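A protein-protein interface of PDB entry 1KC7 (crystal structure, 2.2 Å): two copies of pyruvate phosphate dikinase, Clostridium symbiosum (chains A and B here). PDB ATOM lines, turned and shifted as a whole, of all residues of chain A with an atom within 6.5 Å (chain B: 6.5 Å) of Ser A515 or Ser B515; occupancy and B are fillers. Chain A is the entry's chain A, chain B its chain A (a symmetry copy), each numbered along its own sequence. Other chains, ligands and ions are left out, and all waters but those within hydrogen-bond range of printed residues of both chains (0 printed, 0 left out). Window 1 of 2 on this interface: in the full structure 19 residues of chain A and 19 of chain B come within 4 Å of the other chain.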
ATOM      1  N   LEU A 375      19.135 -25.467 -33.821  1.00  0.00           N
ATOM      2  CA  LEU A 375      18.727 -25.015 -32.497  1.00  0.00           C
ATOM      3  C   LEU A 375      18.455 -23.538 -32.378  1.00  0.00           C
ATOM      4  O   LEU A 375      17.796 -23.117 -31.426  1.00  0.00           O
ATOM      5  CB  LEU A 375      19.773 -25.372 -31.454  1.00  0.00           C
ATOM      6  CG  LEU A 375      20.427 -26.751 -31.474  1.00  0.00           C
ATOM      7  CD1 LEU A 375      21.609 -26.755 -30.533  1.00  0.00           C
ATOM      8  CD2 LEU A 375      19.424 -27.815 -31.054  1.00  0.00           C
ATOM      9  N   LEU A 376      18.962 -22.742 -33.311  1.00  0.00           N
ATOM     10  CA  LEU A 376      18.762 -21.293 -33.220  1.00  0.00           C
ATOM     11  C   LEU A 376      17.870 -20.735 -34.282  1.00  0.00           C
ATOM     12  O   LEU A 376      17.784 -19.516 -34.463  1.00  0.00           O
ATOM     13  CB  LEU A 376      20.093 -20.566 -33.245  1.00  0.00           C
ATOM     14  CG  LEU A 376      20.661 -20.438 -31.840  1.00  0.00           C
ATOM     15  CD1 LEU A 376      22.158 -20.239 -31.879  1.00  0.00           C
ATOM     16  CD2 LEU A 376      19.946 -19.287 -31.147  1.00  0.00           C
ATOM     17  N   HIS A 377      17.229 -21.639 -35.009  1.00  0.00           N
ATOM     18  CA  HIS A 377      16.308 -21.236 -36.050  1.00  0.00           C
ATOM     19  C   HIS A 377      15.256 -20.424 -35.336  1.00  0.00           C
ATOM     20  O   HIS A 377      14.755 -20.822 -34.283  1.00  0.00           O
ATOM     21  CB  HIS A 377      15.628 -22.450 -36.679  1.00  0.00           C
ATOM     22  CG  HIS A 377      16.413 -23.066 -37.791  1.00  0.00           C
ATOM     23  ND1 HIS A 377      16.468 -24.427 -38.001  1.00  0.00           N
ATOM     24  CD2 HIS A 377      17.214 -22.507 -38.731  1.00  0.00           C
ATOM     25  CE1 HIS A 377      17.275 -24.680 -39.017  1.00  0.00           C
ATOM     26  NE2 HIS A 377      17.741 -23.533 -39.479  1.00  0.00           N
ATOM     27  N   THR A 379      11.968 -19.451 -33.854  1.00  0.00           N
ATOM     28  CA  THR A 379      10.716 -20.189 -33.659  1.00  0.00           C
ATOM     29  C   THR A 379       9.614 -19.134 -33.727  1.00  0.00           C
ATOM     30  O   THR A 379       9.876 -17.935 -33.691  1.00  0.00           O
ATOM     31  CB  THR A 379      10.650 -20.864 -32.295  1.00  0.00           C
ATOM     32  OG1 THR A 379      10.995 -19.913 -31.285  1.00  0.00           O
ATOM     33  CG2 THR A 379      11.601 -22.071 -32.226  1.00  0.00           C
ATOM     34  N   GLN A 512      10.604 -15.257 -33.533  1.00  0.00           N
ATOM     35  CA  GLN A 512      11.558 -14.569 -32.648  1.00  0.00           C
ATOM     36  C   GLN A 512      12.761 -15.503 -32.392  1.00  0.00           C
ATOM     37  O   GLN A 512      12.890 -16.508 -33.072  1.00  0.00           O
ATOM     38  CB  GLN A 512      10.876 -14.258 -31.330  1.00  0.00           C
ATOM     39  CG  GLN A 512      10.917 -15.422 -30.369  1.00  0.00           C
ATOM     40  CD  GLN A 512       9.732 -15.455 -29.458  1.00  0.00           C
ATOM     41  OE1 GLN A 512       9.736 -16.172 -28.466  1.00  0.00           O
ATOM     42  NE2 GLN A 512       8.693 -14.684 -29.792  1.00  0.00           N
ATOM     43  N   GLU A 513      13.630 -15.215 -31.422  1.00  0.00           N
ATOM     44  CA  GLU A 513      14.783 -16.111 -31.199  1.00  0.00           C
ATOM     45  C   GLU A 513      14.571 -17.380 -30.386  1.00  0.00           C
ATOM     46  O   GLU A 513      14.038 -17.363 -29.287  1.00  0.00           O
ATOM     47  CB  GLU A 513      15.971 -15.388 -30.552  1.00  0.00           C
ATOM     48  CG  GLU A 513      17.134 -16.388 -30.244  1.00  0.00           C
ATOM     49  CD  GLU A 513      18.169 -15.893 -29.218  1.00  0.00           C
ATOM     50  OE1 GLU A 513      19.110 -16.678 -28.912  1.00  0.00           O
ATOM     51  OE2 GLU A 513      18.047 -14.739 -28.721  1.00  0.00           O
ATOM     52  N   ALA A 514      15.048 -18.491 -30.912  1.00  0.00           N
ATOM     53  CA  ALA A 514      14.899 -19.746 -30.193  1.00  0.00           C
ATOM     54  C   ALA A 514      15.553 -19.620 -28.819  1.00  0.00           C
ATOM     55  O   ALA A 514      16.329 -18.710 -28.578  1.00  0.00           O
ATOM     56  CB  ALA A 514      15.542 -20.890 -30.974  1.00  0.00           C
ATOM     57  N   SER A 515      15.215 -20.548 -27.938  1.00  0.00           N
ATOM     58  CA  SER A 515      15.733 -20.610 -26.594  1.00  0.00           C
ATOM     59  C   SER A 515      16.767 -21.737 -26.648  1.00  0.00           C
ATOM     60  O   SER A 515      17.489 -21.839 -27.624  1.00  0.00           O
ATOM     61  CB  SER A 515      14.590 -20.958 -25.640  1.00  0.00           C
ATOM     62  OG  SER A 515      13.478 -20.085 -25.844  1.00  0.00           O
ATOM     63  N   VAL A 516      16.857 -22.582 -25.629  1.00  0.00           N
ATOM     64  CA  VAL A 516      17.832 -23.669 -25.689  1.00  0.00           C
ATOM     65  C   VAL A 516      17.557 -24.849 -24.765  1.00  0.00           C
ATOM     66  O   VAL A 516      17.527 -24.757 -23.543  1.00  0.00           O
ATOM     67  CB  VAL A 516      19.302 -23.172 -25.466  1.00  0.00           C
ATOM     68  CG1 VAL A 516      20.055 -23.128 -26.793  1.00  0.00           C
ATOM     69  CG2 VAL A 516      19.308 -21.781 -24.834  1.00  0.00           C
ATOM     70  N   SER A 517      17.355 -25.988 -25.399  1.00  0.00           N
ATOM     71  CA  SER A 517      17.074 -27.206 -24.690  1.00  0.00           C
ATOM     72  C   SER A 517      18.111 -27.641 -23.688  1.00  0.00           C
ATOM     73  O   SER A 517      19.317 -27.588 -23.948  1.00  0.00           O
ATOM     74  CB  SER A 517      16.887 -28.356 -25.668  1.00  0.00           C
ATOM     75  OG  SER A 517      15.542 -28.425 -26.118  1.00  0.00           O
ATOM     76  N   LEU A 551      26.052 -18.122 -25.400  1.00  0.00           N
ATOM     77  CA  LEU A 551      26.128 -19.456 -26.004  1.00  0.00           C
ATOM     78  C   LEU A 551      27.435 -20.192 -25.753  1.00  0.00           C
ATOM     79  O   LEU A 551      27.633 -21.301 -26.261  1.00  0.00           O
ATOM     80  CB  LEU A 551      25.905 -19.384 -27.494  1.00  0.00           C
ATOM     81  CG  LEU A 551      24.471 -18.997 -27.713  1.00  0.00           C
ATOM     82  CD1 LEU A 551      24.169 -18.778 -29.179  1.00  0.00           C
ATOM     83  CD2 LEU A 551      23.636 -20.134 -27.094  1.00  0.00           C
ATOM     84  N   LEU B 375      11.223 -19.409 -12.291  1.00  0.00           N
ATOM     85  CA  LEU B 375      11.620 -19.848 -13.622  1.00  0.00           C
ATOM     86  C   LEU B 375      10.552 -19.744 -14.678  1.00  0.00           C
ATOM     87  O   LEU B 375      10.871 -19.765 -15.868  1.00  0.00           O
ATOM     88  CB  LEU B 375      12.101 -21.290 -13.598  1.00  0.00           C
ATOM     89  CG  LEU B 375      13.021 -21.767 -12.477  1.00  0.00           C
ATOM     90  CD1 LEU B 375      13.121 -23.274 -12.522  1.00  0.00           C
ATOM     91  CD2 LEU B 375      14.402 -21.150 -12.633  1.00  0.00           C
ATOM     92  N   LEU B 376       9.291 -19.653 -14.272  1.00  0.00           N
ATOM     93  CA  LEU B 376       8.211 -19.591 -15.259  1.00  0.00           C
ATOM     94  C   LEU B 376       7.509 -18.272 -15.311  1.00  0.00           C
ATOM     95  O   LEU B 376       6.450 -18.139 -15.930  1.00  0.00           O
ATOM     96  CB  LEU B 376       7.196 -20.692 -15.012  1.00  0.00           C
ATOM     97  CG  LEU B 376       7.600 -21.966 -15.737  1.00  0.00           C
ATOM     98  CD1 LEU B 376       6.962 -23.177 -15.098  1.00  0.00           C
ATOM     99  CD2 LEU B 376       7.213 -21.817 -17.202  1.00  0.00           C
ATOM    100  N   HIS B 377       8.093 -17.299 -14.624  1.00  0.00           N
ATOM    101  CA  HIS B 377       7.538 -15.962 -14.614  1.00  0.00           C
ATOM    102  C   HIS B 377       7.541 -15.538 -16.062  1.00  0.00           C
ATOM    103  O   HIS B 377       8.531 -15.716 -16.773  1.00  0.00           O
ATOM    104  CB  HIS B 377       8.434 -15.003 -13.834  1.00  0.00           C
ATOM    105  CG  HIS B 377       8.159 -14.989 -12.366  1.00  0.00           C
ATOM    106  ND1 HIS B 377       9.155 -14.866 -11.422  1.00  0.00           N
ATOM    107  CD2 HIS B 377       7.000 -15.125 -11.677  1.00  0.00           C
ATOM    108  CE1 HIS B 377       8.622 -14.937 -10.213  1.00  0.00           C
ATOM    109  NE2 HIS B 377       7.316 -15.093 -10.339  1.00  0.00           N
ATOM    110  N   THR B 379       8.467 -13.727 -19.195  1.00  0.00           N
ATOM    111  CA  THR B 379       9.549 -12.788 -19.509  1.00  0.00           C
ATOM    112  C   THR B 379       8.988 -11.882 -20.605  1.00  0.00           C
ATOM    113  O   THR B 379       7.944 -12.159 -21.187  1.00  0.00           O
ATOM    114  CB  THR B 379      10.784 -13.491 -20.056  1.00  0.00           C
ATOM    115  OG1 THR B 379      10.390 -14.385 -21.100  1.00  0.00           O
ATOM    116  CG2 THR B 379      11.516 -14.268 -18.949  1.00  0.00           C
ATOM    117  N   GLN B 512       5.605 -12.938 -22.472  1.00  0.00           N
ATOM    118  CA  GLN B 512       5.180 -14.250 -22.987  1.00  0.00           C
ATOM    119  C   GLN B 512       5.702 -15.349 -22.037  1.00  0.00           C
ATOM    120  O   GLN B 512       6.155 -15.031 -20.950  1.00  0.00           O
ATOM    121  CB  GLN B 512       5.773 -14.457 -24.367  1.00  0.00           C
ATOM    122  CG  GLN B 512       7.181 -15.000 -24.315  1.00  0.00           C
ATOM    123  CD  GLN B 512       8.012 -14.551 -25.473  1.00  0.00           C
ATOM    124  OE1 GLN B 512       9.081 -15.097 -25.715  1.00  0.00           O
ATOM    125  NE2 GLN B 512       7.536 -13.534 -26.198  1.00  0.00           N
ATOM    126  N   GLU B 513       5.671 -16.627 -22.420  1.00  0.00           N
ATOM    127  CA  GLU B 513       6.162 -17.668 -21.494  1.00  0.00           C
ATOM    128  C   GLU B 513       7.661 -17.916 -21.407  1.00  0.00           C
ATOM    129  O   GLU B 513       8.344 -18.109 -22.402  1.00  0.00           O
ATOM    130  CB  GLU B 513       5.521 -19.036 -21.758  1.00  0.00           C
ATOM    131  CG  GLU B 513       6.136 -20.131 -20.824  1.00  0.00           C
ATOM    132  CD  GLU B 513       5.913 -21.583 -21.282  1.00  0.00           C
ATOM    133  OE1 GLU B 513       6.417 -22.502 -20.578  1.00  0.00           O
ATOM    134  OE2 GLU B 513       5.246 -21.807 -22.330  1.00  0.00           O
ATOM    135  N   ALA B 514       8.170 -17.967 -20.192  1.00  0.00           N
ATOM    136  CA  ALA B 514       9.593 -18.214 -20.020  1.00  0.00           C
ATOM    137  C   ALA B 514       9.957 -19.541 -20.682  1.00  0.00           C
ATOM    138  O   ALA B 514       9.092 -20.346 -20.986  1.00  0.00           O
ATOM    139  CB  ALA B 514       9.954 -18.254 -18.537  1.00  0.00           C
ATOM    140  N   SER B 515      11.249 -19.737 -20.896  1.00  0.00           N
ATOM    141  CA  SER B 515      11.794 -20.928 -21.497  1.00  0.00           C
ATOM    142  C   SER B 515      12.375 -21.705 -20.314  1.00  0.00           C
ATOM    143  O   SER B 515      11.765 -21.734 -19.260  1.00  0.00           O
ATOM    144  CB  SER B 515      12.891 -20.526 -22.483  1.00  0.00           C
ATOM    145  OG  SER B 515      12.417 -19.529 -23.388  1.00  0.00           O
ATOM    146  N   VAL B 516      13.535 -22.333 -20.459  1.00  0.00           N
ATOM    147  CA  VAL B 516      14.099 -23.060 -19.324  1.00  0.00           C
ATOM    148  C   VAL B 516      15.598 -23.323 -19.391  1.00  0.00           C
ATOM    149  O   VAL B 516      16.126 -24.002 -20.265  1.00  0.00           O
ATOM    150  CB  VAL B 516      13.351 -24.409 -19.041  1.00  0.00           C
ATOM    151  CG1 VAL B 516      12.441 -24.268 -17.824  1.00  0.00           C
ATOM    152  CG2 VAL B 516      12.517 -24.824 -20.252  1.00  0.00           C
ATOM    153  N   SER B 517      16.284 -22.756 -18.418  1.00  0.00           N
ATOM    154  CA  SER B 517      17.713 -22.890 -18.326  1.00  0.00           C
ATOM    155  C   SER B 517      18.239 -24.298 -18.235  1.00  0.00           C
ATOM    156  O   SER B 517      17.701 -25.139 -17.507  1.00  0.00           O
ATOM    157  CB  SER B 517      18.236 -22.137 -17.112  1.00  0.00           C
ATOM    158  OG  SER B 517      18.485 -20.776 -17.429  1.00  0.00           O
ATOM    159  N   LEU B 551       7.187 -30.149 -18.698  1.00  0.00           N
ATOM    160  CA  LEU B 551       7.963 -29.820 -17.497  1.00  0.00           C
ATOM    161  C   LEU B 551       8.289 -31.009 -16.608  1.00  0.00           C
ATOM    162  O   LEU B 551       8.890 -30.842 -15.541  1.00  0.00           O
ATOM    163  CB  LEU B 551       7.249 -28.787 -16.663  1.00  0.00           C
ATOM    164  CG  LEU B 551       7.262 -27.500 -17.437  1.00  0.00           C
ATOM    165  CD1 LEU B 551       6.463 -26.421 -16.741  1.00  0.00           C
ATOM    166  CD2 LEU B 551       8.749 -27.131 -17.600  1.00  0.00           C
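OE1 of Gln A512 sits close to OE1 of Gln B512 (3.0 Å). OG of Ser B515 lies within hydrogen-bond range of OG of Ser A515 (2.7 Å).
The backbone carbonyl oxygen (O) of Thr A379 is in hydrogen-bond range of the backbone NH (N) of Gln A512 (2.8 Å). O of Thr B379 lies within hydrogen-bond range of N of Gln B512.
Among the printed residues, merely in contact across the chains: Val A516 with Val B516 (3.6 Å).
Ser A515 touches just one residue of chain B: Ser B515 (2.7 Å). Printed residues of chain B within 4 Å of Val A516: Val B516 (3.6 Å). Leu A551 touches none of the printed residues of chain B. Leu B376 touches none of the printed residues of chain A. Printed residues of chain A within 4 Å of Gln B512: Gln A512. Ser B515 touches one residue of chain A. Printed residues of chain A within 4 Å of Val B516: Val A516. The nearest printed residue of chain B that does not touch Val A516 is Ser B517 (5.4 Å).
Of the 11 printed residues of chain B, 3 touch a printed residue of chain A. Along chain A the printed residues that touch a printed residue of chain B span positions 512 to 516.
Gln B512 touches its own counterpart, Gln A512. Ser B515 touches its own counterpart, Ser A515. Val A516 touches its own counterpart, Val B516. Of the 3 pairs that touch across the chains among the printed residues, 3 have their exchanged pair printed and touching as well.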
